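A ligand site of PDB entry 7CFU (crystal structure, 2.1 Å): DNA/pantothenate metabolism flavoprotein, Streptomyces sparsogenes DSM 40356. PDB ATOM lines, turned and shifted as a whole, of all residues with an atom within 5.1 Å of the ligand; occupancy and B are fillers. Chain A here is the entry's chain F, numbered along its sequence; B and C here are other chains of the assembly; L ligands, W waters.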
ATOM      1  N   CYS A  29     -15.537 -23.156 -19.576  1.00  0.00           N
ATOM      2  CA  CYS A  29     -15.300 -22.009 -20.440  1.00  0.00           C
ATOM      3  C   CYS A  29     -13.819 -21.626 -20.393  1.00  0.00           C
ATOM      4  O   CYS A  29     -13.054 -22.097 -19.557  1.00  0.00           O
ATOM      5  CB  CYS A  29     -16.172 -20.825 -20.009  1.00  0.00           C
ATOM      6  SG  CYS A  29     -17.942 -21.188 -19.988  1.00  0.00           S
ATOM      7  N   GLY A  30     -13.437 -20.754 -21.331  1.00  0.00           N
ATOM      8  CA  GLY A  30     -12.043 -20.358 -21.482  1.00  0.00           C
ATOM      9  C   GLY A  30     -11.587 -19.335 -20.454  1.00  0.00           C
ATOM     10  O   GLY A  30     -11.376 -18.165 -20.788  1.00  0.00           O
ATOM     11  N   SER A  31     -11.444 -19.774 -19.206  1.00  0.00           N
ATOM     12  CA  SER A  31     -10.997 -18.923 -18.101  1.00  0.00           C
ATOM     13  C   SER A  31      -9.677 -19.456 -17.552  1.00  0.00           C
ATOM     14  O   SER A  31      -9.396 -20.653 -17.650  1.00  0.00           O
ATOM     15  CB  SER A  31     -12.052 -18.881 -16.982  1.00  0.00           C
ATOM     16  OG  SER A  31     -11.478 -18.501 -15.735  1.00  0.00           O
ATOM     17  N   PHE A  32      -8.869 -18.564 -16.959  1.00  0.00           N
ATOM     18  CA  PHE A  32      -7.687 -18.992 -16.208  1.00  0.00           C
ATOM     19  C   PHE A  32      -8.010 -20.149 -15.271  1.00  0.00           C
ATOM     20  O   PHE A  32      -7.180 -21.041 -15.058  1.00  0.00           O
ATOM     21  CB  PHE A  32      -7.106 -17.854 -15.369  1.00  0.00           C
ATOM     22  CG  PHE A  32      -6.361 -16.816 -16.154  1.00  0.00           C
ATOM     23  CD1 PHE A  32      -5.115 -17.115 -16.700  1.00  0.00           C
ATOM     24  CD2 PHE A  32      -6.861 -15.549 -16.303  1.00  0.00           C
ATOM     25  CE1 PHE A  32      -4.408 -16.162 -17.399  1.00  0.00           C
ATOM     26  CE2 PHE A  32      -6.165 -14.586 -17.003  1.00  0.00           C
ATOM     27  CZ  PHE A  32      -4.928 -14.887 -17.560  1.00  0.00           C
ATOM     28  N   SER A  33      -9.192 -20.135 -14.654  1.00  0.00           N
ATOM     29  CA  SER A  33      -9.525 -21.143 -13.665  1.00  0.00           C
ATOM     30  C   SER A  33      -9.840 -22.508 -14.266  1.00  0.00           C
ATOM     31  O   SER A  33     -10.164 -23.422 -13.495  1.00  0.00           O
ATOM     32  CB  SER A  33     -10.693 -20.668 -12.808  1.00  0.00           C
ATOM     33  OG  SER A  33     -10.286 -19.587 -11.994  1.00  0.00           O
ATOM     34  N   THR A  58     -16.158 -25.009 -24.273  1.00  0.00           N
ATOM     35  CA  THR A  58     -16.202 -24.019 -25.334  1.00  0.00           C
ATOM     36  C   THR A  58     -14.974 -24.166 -26.220  1.00  0.00           C
ATOM     37  O   THR A  58     -13.973 -24.791 -25.838  1.00  0.00           O
ATOM     38  CB  THR A  58     -16.273 -22.604 -24.753  1.00  0.00           C
ATOM     39  OG1 THR A  58     -15.018 -22.259 -24.134  1.00  0.00           O
ATOM     40  CG2 THR A  58     -17.364 -22.534 -23.727  1.00  0.00           C
ATOM     41  N   GLN A  60     -12.930 -21.900 -26.888  1.00  0.00           N
ATOM     42  CA  GLN A  60     -11.824 -21.219 -26.225  1.00  0.00           C
ATOM     43  C   GLN A  60     -11.225 -22.072 -25.107  1.00  0.00           C
ATOM     44  O   GLN A  60      -9.998 -22.148 -24.969  1.00  0.00           O
ATOM     45  CB  GLN A  60     -12.301 -19.865 -25.669  1.00  0.00           C
ATOM     46  CG  GLN A  60     -11.253 -19.131 -24.859  1.00  0.00           C
ATOM     47  CD  GLN A  60     -10.224 -18.415 -25.736  1.00  0.00           C
ATOM     48  OE1 GLN A  60      -9.937 -18.838 -26.854  1.00  0.00           O
ATOM     49  NE2 GLN A  60      -9.694 -17.309 -25.223  1.00  0.00           N
ATOM     50  N   ALA A  61     -12.062 -22.728 -24.303  1.00  0.00           N
ATOM     51  CA  ALA A  61     -11.529 -23.637 -23.282  1.00  0.00           C
ATOM     52  C   ALA A  61     -10.680 -24.721 -23.924  1.00  0.00           C
ATOM     53  O   ALA A  61      -9.579 -25.024 -23.449  1.00  0.00           O
ATOM     54  CB  ALA A  61     -12.682 -24.255 -22.483  1.00  0.00           C
ATOM     55  N   LEU A  64      -7.217 -23.410 -25.086  1.00  0.00           N
ATOM     56  CA  LEU A  64      -6.300 -23.094 -24.003  1.00  0.00           C
ATOM     57  C   LEU A  64      -5.847 -24.361 -23.285  1.00  0.00           C
ATOM     58  O   LEU A  64      -4.657 -24.552 -23.051  1.00  0.00           O
ATOM     59  CB  LEU A  64      -6.974 -22.146 -23.008  1.00  0.00           C
ATOM     60  CG  LEU A  64      -7.351 -20.773 -23.547  1.00  0.00           C
ATOM     61  CD1 LEU A  64      -7.991 -19.944 -22.450  1.00  0.00           C
ATOM     62  CD2 LEU A  64      -6.106 -20.087 -24.086  1.00  0.00           C
ATOM     63  N   ALA A 107     -16.991 -20.366 -15.441  1.00  0.00           N
ATOM     64  CA  ALA A 107     -17.729 -19.629 -16.442  1.00  0.00           C
ATOM     65  C   ALA A 107     -16.989 -18.334 -16.741  1.00  0.00           C
ATOM     66  O   ALA A 107     -16.388 -17.737 -15.849  1.00  0.00           O
ATOM     67  CB  ALA A 107     -19.159 -19.338 -15.981  1.00  0.00           C
ATOM     68  N   THR A 108     -17.008 -17.923 -18.000  1.00  0.00           N
ATOM     69  CA  THR A 108     -16.453 -16.636 -18.364  1.00  0.00           C
ATOM     70  C   THR A 108     -17.522 -15.561 -18.232  1.00  0.00           C
ATOM     71  O   THR A 108     -18.718 -15.855 -18.163  1.00  0.00           O
ATOM     72  CB  THR A 108     -15.949 -16.652 -19.799  1.00  0.00           C
ATOM     73  OG1 THR A 108     -16.983 -17.224 -20.615  1.00  0.00           O
ATOM     74  CG2 THR A 108     -14.664 -17.495 -19.910  1.00  0.00           C
ATOM     75  N   ALA A 109     -17.069 -14.298 -18.194  1.00  0.00           N
ATOM     76  CA  ALA A 109     -18.005 -13.197 -18.351  1.00  0.00           C
ATOM     77  C   ALA A 109     -18.801 -13.348 -19.642  1.00  0.00           C
ATOM     78  O   ALA A 109     -20.012 -13.120 -19.667  1.00  0.00           O
ATOM     79  CB  ALA A 109     -17.256 -11.853 -18.337  1.00  0.00           C
ATOM     80  N   ASN A 110     -18.133 -13.772 -20.719  1.00  0.00           N
ATOM     81  CA  ASN A 110     -18.808 -14.042 -21.983  1.00  0.00           C
ATOM     82  C   ASN A 110     -19.967 -14.997 -21.792  1.00  0.00           C
ATOM     83  O   ASN A 110     -21.078 -14.765 -22.300  1.00  0.00           O
ATOM     84  CB  ASN A 110     -17.799 -14.623 -22.975  1.00  0.00           C
ATOM     85  CG  ASN A 110     -18.355 -14.758 -24.377  1.00  0.00           C
ATOM     86  OD1 ASN A 110     -18.929 -13.817 -24.939  1.00  0.00           O
ATOM     87  ND2 ASN A 110     -18.205 -15.964 -24.947  1.00  0.00           N
ATOM     88  N   PHE A 111     -19.734 -16.095 -21.060  1.00  0.00           N
ATOM     89  CA  PHE A 111     -20.807 -17.052 -20.812  1.00  0.00           C
ATOM     90  C   PHE A 111     -21.990 -16.416 -20.094  1.00  0.00           C
ATOM     91  O   PHE A 111     -23.155 -16.683 -20.444  1.00  0.00           O
ATOM     92  CB  PHE A 111     -20.288 -18.252 -19.998  1.00  0.00           C
ATOM     93  CG  PHE A 111     -21.382 -19.202 -19.631  1.00  0.00           C
ATOM     94  CD1 PHE A 111     -22.029 -19.089 -18.407  1.00  0.00           C
ATOM     95  CD2 PHE A 111     -21.804 -20.173 -20.525  1.00  0.00           C
ATOM     96  CE1 PHE A 111     -23.068 -19.952 -18.075  1.00  0.00           C
ATOM     97  CE2 PHE A 111     -22.832 -21.035 -20.201  1.00  0.00           C
ATOM     98  CZ  PHE A 111     -23.460 -20.919 -18.976  1.00  0.00           C
ATOM     99  N   LYS A 114     -24.089 -14.579 -22.591  1.00  0.00           N
ATOM    100  CA  LYS A 114     -24.855 -15.434 -23.491  1.00  0.00           C
ATOM    101  C   LYS A 114     -25.995 -16.130 -22.752  1.00  0.00           C
ATOM    102  O   LYS A 114     -27.131 -16.162 -23.246  1.00  0.00           O
ATOM    103  CB  LYS A 114     -23.920 -16.458 -24.145  1.00  0.00           C
ATOM    104  CG  LYS A 114     -22.939 -15.866 -25.149  1.00  0.00           C
ATOM    105  CD  LYS A 114     -22.032 -16.964 -25.736  1.00  0.00           C
ATOM    106  CE  LYS A 114     -21.121 -16.398 -26.837  1.00  0.00           C
ATOM    107  NZ  LYS A 114     -20.212 -17.446 -27.383  1.00  0.00           N
ATOM    108  N   ASP A 122     -23.041 -21.929 -29.596  1.00  0.00           N
ATOM    109  CA  ASP A 122     -22.159 -23.085 -29.564  1.00  0.00           C
ATOM    110  C   ASP A 122     -22.879 -24.182 -28.778  1.00  0.00           C
ATOM    111  O   ASP A 122     -23.983 -23.968 -28.262  1.00  0.00           O
ATOM    112  CB  ASP A 122     -20.790 -22.759 -28.966  1.00  0.00           C
ATOM    113  CG  ASP A 122     -20.844 -22.345 -27.488  1.00  0.00           C
ATOM    114  OD1 ASP A 122     -21.938 -22.282 -26.893  1.00  0.00           O
ATOM    115  OD2 ASP A 122     -19.756 -22.098 -26.914  1.00  0.00           O
ATOM    116  N   VAL A 140     -15.550 -16.679 -13.265  1.00  0.00           N
ATOM    117  CA  VAL A 140     -14.233 -16.185 -12.848  1.00  0.00           C
ATOM    118  C   VAL A 140     -13.777 -15.115 -13.826  1.00  0.00           C
ATOM    119  O   VAL A 140     -13.891 -15.286 -15.043  1.00  0.00           O
ATOM    120  CB  VAL A 140     -13.197 -17.316 -12.763  1.00  0.00           C
ATOM    121  CG1 VAL A 140     -11.872 -16.752 -12.285  1.00  0.00           C
ATOM    122  CG2 VAL A 140     -13.676 -18.419 -11.838  1.00  0.00           C
ATOM    123  N   MET A 141     -13.258 -14.021 -13.284  1.00  0.00           N
ATOM    124  CA  MET A 141     -12.744 -12.895 -14.056  1.00  0.00           C
ATOM    125  C   MET A 141     -12.065 -11.950 -13.071  1.00  0.00           C
ATOM    126  O   MET A 141     -12.243 -12.079 -11.854  1.00  0.00           O
ATOM    127  CB  MET A 141     -13.854 -12.168 -14.816  1.00  0.00           C
ATOM    128  CG  MET A 141     -14.824 -11.401 -13.918  1.00  0.00           C
ATOM    129  SD  MET A 141     -16.383 -10.971 -14.740  1.00  0.00           S
ATOM    130  CE  MET A 141     -17.207 -12.554 -14.653  1.00  0.00           C
ATOM    131  N   MET A 145     -13.396  -6.503 -14.662  1.00  0.00           N
ATOM    132  CA  MET A 145     -14.470  -7.099 -15.451  1.00  0.00           C
ATOM    133  C   MET A 145     -15.704  -7.364 -14.593  1.00  0.00           C
ATOM    134  O   MET A 145     -16.828  -7.094 -15.000  1.00  0.00           O
ATOM    135  CB  MET A 145     -13.970  -8.399 -16.105  1.00  0.00           C
ATOM    136  CG  MET A 145     -12.734  -8.224 -17.005  1.00  0.00           C
ATOM    137  SD  MET A 145     -11.913  -9.784 -17.447  1.00  0.00           S
ATOM    138  CE  MET A 145     -13.194 -10.551 -18.447  1.00  0.00           C
ATOM    139  N   TRP B  82      -6.048 -14.152 -29.649  1.00  0.00           N
ATOM    140  CA  TRP B  82      -5.454 -14.323 -28.329  1.00  0.00           C
ATOM    141  C   TRP B  82      -3.974 -14.623 -28.415  1.00  0.00           C
ATOM    142  O   TRP B  82      -3.194 -14.148 -27.581  1.00  0.00           O
ATOM    143  CB  TRP B  82      -6.168 -15.449 -27.584  1.00  0.00           C
ATOM    144  CG  TRP B  82      -7.602 -15.135 -27.454  1.00  0.00           C
ATOM    145  CD1 TRP B  82      -8.620 -15.625 -28.207  1.00  0.00           C
ATOM    146  CD2 TRP B  82      -8.177 -14.197 -26.541  1.00  0.00           C
ATOM    147  NE1 TRP B  82      -9.809 -15.067 -27.813  1.00  0.00           N
ATOM    148  CE2 TRP B  82      -9.559 -14.186 -26.794  1.00  0.00           C
ATOM    149  CE3 TRP B  82      -7.658 -13.378 -25.542  1.00  0.00           C
ATOM    150  CZ2 TRP B  82     -10.448 -13.389 -26.060  1.00  0.00           C
ATOM    151  CZ3 TRP B  82      -8.534 -12.590 -24.817  1.00  0.00           C
ATOM    152  CH2 TRP B  82      -9.904 -12.597 -25.079  1.00  0.00           C
ATOM    153  N   GLY B  89      -0.482 -13.950 -18.447  1.00  0.00           N
ATOM    154  CA  GLY B  89      -1.767 -13.247 -18.529  1.00  0.00           C
ATOM    155  C   GLY B  89      -2.497 -13.552 -19.818  1.00  0.00           C
ATOM    156  O   GLY B  89      -2.638 -14.709 -20.211  1.00  0.00           O
ATOM    157  N   ALA B  90      -2.877 -12.499 -20.543  1.00  0.00           N
ATOM    158  CA  ALA B  90      -3.877 -12.612 -21.600  1.00  0.00           C
ATOM    159  C   ALA B  90      -4.113 -11.253 -22.248  1.00  0.00           C
ATOM    160  O   ALA B  90      -4.011 -10.213 -21.590  1.00  0.00           O
ATOM    161  CB  ALA B  90      -5.189 -13.164 -21.033  1.00  0.00           C
ATOM    162  N   HIS B  92      -6.576  -9.386 -23.299  1.00  0.00           N
ATOM    163  CA  HIS B  92      -7.560  -8.385 -22.880  1.00  0.00           C
ATOM    164  C   HIS B  92      -7.152  -7.721 -21.571  1.00  0.00           C
ATOM    165  O   HIS B  92      -7.380  -6.520 -21.388  1.00  0.00           O
ATOM    166  CB  HIS B  92      -8.957  -9.012 -22.783  1.00  0.00           C
ATOM    167  CG  HIS B  92      -9.076 -10.079 -21.737  1.00  0.00           C
ATOM    168  ND1 HIS B  92      -8.225 -11.158 -21.677  1.00  0.00           N
ATOM    169  CD2 HIS B  92      -9.943 -10.227 -20.707  1.00  0.00           C
ATOM    170  CE1 HIS B  92      -8.564 -11.926 -20.654  1.00  0.00           C
ATOM    171  NE2 HIS B  92      -9.607 -11.385 -20.047  1.00  0.00           N
ATOM    172  N   ALA B 120     -18.272 -10.938 -24.605  1.00  0.00           N
ATOM    173  CA  ALA B 120     -16.824 -10.888 -24.728  1.00  0.00           C
ATOM    174  C   ALA B 120     -16.343 -12.119 -25.493  1.00  0.00           C
ATOM    175  O   ALA B 120     -15.656 -12.978 -24.940  1.00  0.00           O
ATOM    176  CB  ALA B 120     -16.149 -10.811 -23.357  1.00  0.00           C
ATOM    177  N   ASP B 121     -16.720 -12.227 -26.779  1.00  0.00           N
ATOM    178  CA  ASP B 121     -16.403 -13.424 -27.547  1.00  0.00           C
ATOM    179  C   ASP B 121     -15.263 -13.208 -28.544  1.00  0.00           C
ATOM    180  O   ASP B 121     -15.062 -14.064 -29.426  1.00  0.00           O
ATOM    181  CB  ASP B 121     -17.652 -13.958 -28.249  1.00  0.00           C
ATOM    182  CG  ASP B 121     -18.252 -12.986 -29.265  1.00  0.00           C
ATOM    183  OD1 ASP B 121     -17.715 -11.863 -29.453  1.00  0.00           O
ATOM    184  OD2 ASP B 121     -19.296 -13.339 -29.857  1.00  0.00           O
ATOM    185  N   ASP B 122     -14.518 -12.107 -28.425  1.00  0.00           N
ATOM    186  CA  ASP B 122     -13.247 -11.940 -29.112  1.00  0.00           C
ATOM    187  C   ASP B 122     -12.363 -11.012 -28.271  1.00  0.00           C
ATOM    188  O   ASP B 122     -12.771 -10.551 -27.203  1.00  0.00           O
ATOM    189  CB  ASP B 122     -13.453 -11.426 -30.554  1.00  0.00           C
ATOM    190  CG  ASP B 122     -14.054 -10.019 -30.629  1.00  0.00           C
ATOM    191  OD1 ASP B 122     -14.336  -9.384 -29.588  1.00  0.00           O
ATOM    192  OD2 ASP B 122     -14.269  -9.549 -31.773  1.00  0.00           O
ATOM    193  N   ALA B 126     -13.689  -8.482 -25.115  1.00  0.00           N
ATOM    194  CA  ALA B 126     -13.168  -8.832 -23.794  1.00  0.00           C
ATOM    195  C   ALA B 126     -12.310  -7.703 -23.244  1.00  0.00           C
ATOM    196  O   ALA B 126     -12.295  -7.451 -22.034  1.00  0.00           O
ATOM    197  CB  ALA B 126     -12.375 -10.128 -23.852  1.00  0.00           C
ATOM    198  N   MET C  69      -2.099 -22.337 -22.083  1.00  0.00           N
ATOM    199  CA  MET C  69      -2.389 -22.008 -20.687  1.00  0.00           C
ATOM    200  C   MET C  69      -1.106 -22.014 -19.860  1.00  0.00           C
ATOM    201  O   MET C  69      -0.913 -21.137 -19.007  1.00  0.00           O
ATOM    202  CB  MET C  69      -3.397 -22.991 -20.093  1.00  0.00           C
ATOM    203  CG  MET C  69      -3.824 -22.625 -18.676  1.00  0.00           C
ATOM    204  SD  MET C  69      -4.623 -20.999 -18.583  1.00  0.00           S
ATOM    205  CE  MET C  69      -6.329 -21.555 -18.731  1.00  0.00           C
ATOM    206  N   ALA C  72       0.375 -18.792 -20.267  1.00  0.00           N
ATOM    207  CA  ALA C  72      -0.355 -17.727 -19.585  1.00  0.00           C
ATOM    208  C   ALA C  72      -0.069 -17.701 -18.077  1.00  0.00           C
ATOM    209  O   ALA C  72      -0.138 -16.638 -17.462  1.00  0.00           O
ATOM    210  CB  ALA C  72      -1.854 -17.848 -19.849  1.00  0.00           C
HETATM  211  N1  LIG L   1     -12.387 -14.308 -19.540  1.00  0.00           N
HETATM  212  C1  LIG L   1     -13.092 -14.291 -18.362  1.00  0.00           C
HETATM  213  O1  LIG L   1     -14.212 -13.803 -18.345  1.00  0.00           O
HETATM  214  N2  LIG L   1     -12.549 -14.818 -17.204  1.00  0.00           N
HETATM  215  C2  LIG L   1     -11.281 -15.361 -17.230  1.00  0.00           C
HETATM  216  O2  LIG L   1     -10.794 -15.833 -16.206  1.00  0.00           O
HETATM  217  C3  LIG L   1     -10.566 -15.378 -18.417  1.00  0.00           C
HETATM  218  N3  LIG L   1      -9.305 -15.932 -18.465  1.00  0.00           N
HETATM  219  C4  LIG L   1      -8.608 -15.960 -19.663  1.00  0.00           C
HETATM  220  C5  LIG L   1      -7.339 -16.513 -19.690  1.00  0.00           C
HETATM  221  C6  LIG L   1      -6.622 -16.550 -20.876  1.00  0.00           C
HETATM  222  C7  LIG L   1      -5.247 -17.152 -20.906  1.00  0.00           C
HETATM  223  C8  LIG L   1      -7.175 -16.013 -22.036  1.00  0.00           C
HETATM  224  C9  LIG L   1      -6.379 -16.051 -23.317  1.00  0.00           C
HETATM  225  C10 LIG L   1      -8.455 -15.451 -22.010  1.00  0.00           C
HETATM  226  C11 LIG L   1      -9.162 -15.424 -20.812  1.00  0.00           C
HETATM  227  N4  LIG L   1     -10.435 -14.861 -20.756  1.00  0.00           N
HETATM  228  C12 LIG L   1     -11.128 -14.852 -19.577  1.00  0.00           C
HETATM  229  C13 LIG L   1     -11.067 -14.292 -21.981  1.00  0.00           C
HETATM  230  C14 LIG L   1     -11.989 -15.347 -22.576  1.00  0.00           C
HETATM  231  O3  LIG L   1     -11.251 -16.525 -22.857  1.00  0.00           O
HETATM  232  C15 LIG L   1     -12.692 -14.775 -23.807  1.00  0.00           C
HETATM  233  O4  LIG L   1     -13.624 -13.788 -23.394  1.00  0.00           O
HETATM  234  C16 LIG L   1     -13.358 -15.851 -24.672  1.00  0.00           C
HETATM  235  O5  LIG L   1     -13.952 -15.238 -25.804  1.00  0.00           O
HETATM  236  C17 LIG L   1     -14.425 -16.601 -23.889  1.00  0.00           C
HETATM  237  O6  LIG L   1     -14.854 -17.714 -24.645  1.00  0.00           O
HETATM  238  P1  LIG L   1     -15.948 -18.736 -24.069  1.00  0.00           P
HETATM  239  O7  LIG L   1     -16.801 -19.236 -25.210  1.00  0.00           O
HETATM  240  O8  LIG L   1     -15.214 -19.803 -23.335  1.00  0.00           O
HETATM  241  O9  LIG L   1     -16.886 -18.047 -23.089  1.00  0.00           O
HETATM  242  O   HOH W   1      -9.786 -14.271 -13.980  1.00  0.00           O
HETATM  243  O   HOH W   2     -19.200 -19.720 -25.604  1.00  0.00           O
HETATM  244  O   HOH W   3     -19.362 -19.389 -22.832  1.00  0.00           O
HETATM  245  O   HOH W   4     -12.543 -15.697 -28.115  1.00  0.00           O
HETATM  246  O   HOH W   5     -15.367 -13.386 -20.870  1.00  0.00           O
HETATM  247  O   HOH W   6     -15.423 -20.373 -27.295  1.00  0.00           O
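The backbone carbonyl oxygen (O) of Val 140 sits at hydrogen-bond distance from a nitrogen (N2) of the ligand (2.6 Å).
The backbone carbonyl oxygen of Ala 120 of chain B is in hydrogen-bond range of an oxygen (O4) of the ligand, 2.7 Å away.
An oxygen (O2) of the ligand lies within hydrogen-bond range of the side-chain hydroxyl (OG) of Ser 31, at 2.8 Å.
An oxygen (O8) of the ligand is in hydrogen-bond range of the backbone NH (N) of Gly 30, 2.8 Å away.
The backbone NH (N) of Phe 32 is in hydrogen-bond range of a nitrogen (N3) of the ligand, 3.1 Å away.
The side-chain amide nitrogen (NE2) of Gln 60 sits at hydrogen-bond distance from an oxygen (O3) of the ligand.
The side-chain hydroxyl of Thr 108 sits at hydrogen-bond distance from an oxygen (O9) of the ligand (2.6 Å).
O1 of the ligand is in hydrogen-bond range of N of Ala 109 (2.9 Å).
ND2 of Asn 110 lies within hydrogen-bond range of O9 of the ligand, 3.1 Å away.
An oxygen (O8) of the ligand lies within hydrogen-bond range of the side-chain hydroxyl (OG1) of Thr 58 (2.6 Å).
An oxygen (O3) of the ligand sits at hydrogen-bond distance from the backbone carbonyl oxygen of Gly 30.
Cys 29 touches the ligand.
Leu 64 touches the ligand.
CA of Met 141 touches N2 of the ligand (3.7 Å).
Met 145 touches the ligand (CE to O1, 3.4 Å).
Trp 82 of chain B touches the ligand.
O of Gly 89 of chain B touches C7 of the ligand, at 3.6 Å.
CB of Ala 90 of chain B touches C8 of the ligand (3.6 Å).
His 92 of chain B touches the ligand (CE1 to N4, 3.5 Å).
Asp 121 of chain B touches the ligand (CA to O5, 3.5 Å).
CB of Ala 126 of chain B touches O4 of the ligand, at 3.9 Å.
CB of Ala 72 of chain C touches C7 of the ligand (3.6 Å).
Hydrophobic or aromatic side chains within 4 Å of the ligand: Phe 32, Leu 64, Ala 109, Met 141, Met 145, Trp 82 of chain B, Ala 90 of chain B, His 92 of chain B, Ala 120 of chain B, Ala 126 of chain B and Ala 72 of chain C.
OD1 of Asn 110 lies within hydrogen-bond range of N of Asp 121 of chain B, 3.3 Å away.
The backbone NH (N) of Ser 33 sits at hydrogen-bond distance from the side-chain hydroxyl (OG) of Ser 31, 3.0 Å away.
The backbone NH (N) of Ala 61 is in hydrogen-bond range of the side-chain hydroxyl (OG1) of Thr 58 (3.0 Å).
NE2 of Gln 60 lies close to NE1 of Trp 82 of chain B, at 3.4 Å.
The backbone NH of Val 140 is in hydrogen-bond range of the backbone carbonyl oxygen of Ala 107, at 2.9 Å.
The side-chain amide oxygen (OD1) of Asn 110 is in hydrogen-bond range of the backbone NH (N) of Ala 120 of chain B, 3.0 Å away.
N of Phe 111 is in hydrogen-bond range of OG1 of Thr 108 (3.0 Å).
The side-chain hydroxyl (OG1) of Thr 58 lies close to the backbone NH (N) of Gln 60 (3.5 Å).
Water W2 lies within hydrogen-bond range of an oxygen (O7) of the ligand, the side-chain carboxylate (OD2) of Asp 122 of chain A and the side-chain amino group (NZ) of Lys 114.
Water W4 lies within hydrogen-bond range of an oxygen (O5) of the ligand (2.7 Å), the indole nitrogen (NE1) of Trp 82 of chain B (2.8 Å) and the backbone carbonyl oxygen (O) of Asp 121 of chain B (3.3 Å).
Water W6 lies within hydrogen-bond range of O7 of the ligand (2.7 Å) and N of Gln 60 (3.0 Å).
Water W5 lies within hydrogen-bond range of N of Asn 110 (2.8 Å), O1 of the ligand (2.8 Å) and N of Ala 109 (3.3 Å).
Water W3 lies within hydrogen-bond range of an oxygen (O9) of the ligand (2.8 Å) and the side-chain sulfur (SG) of Cys 29 (3.7 Å).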
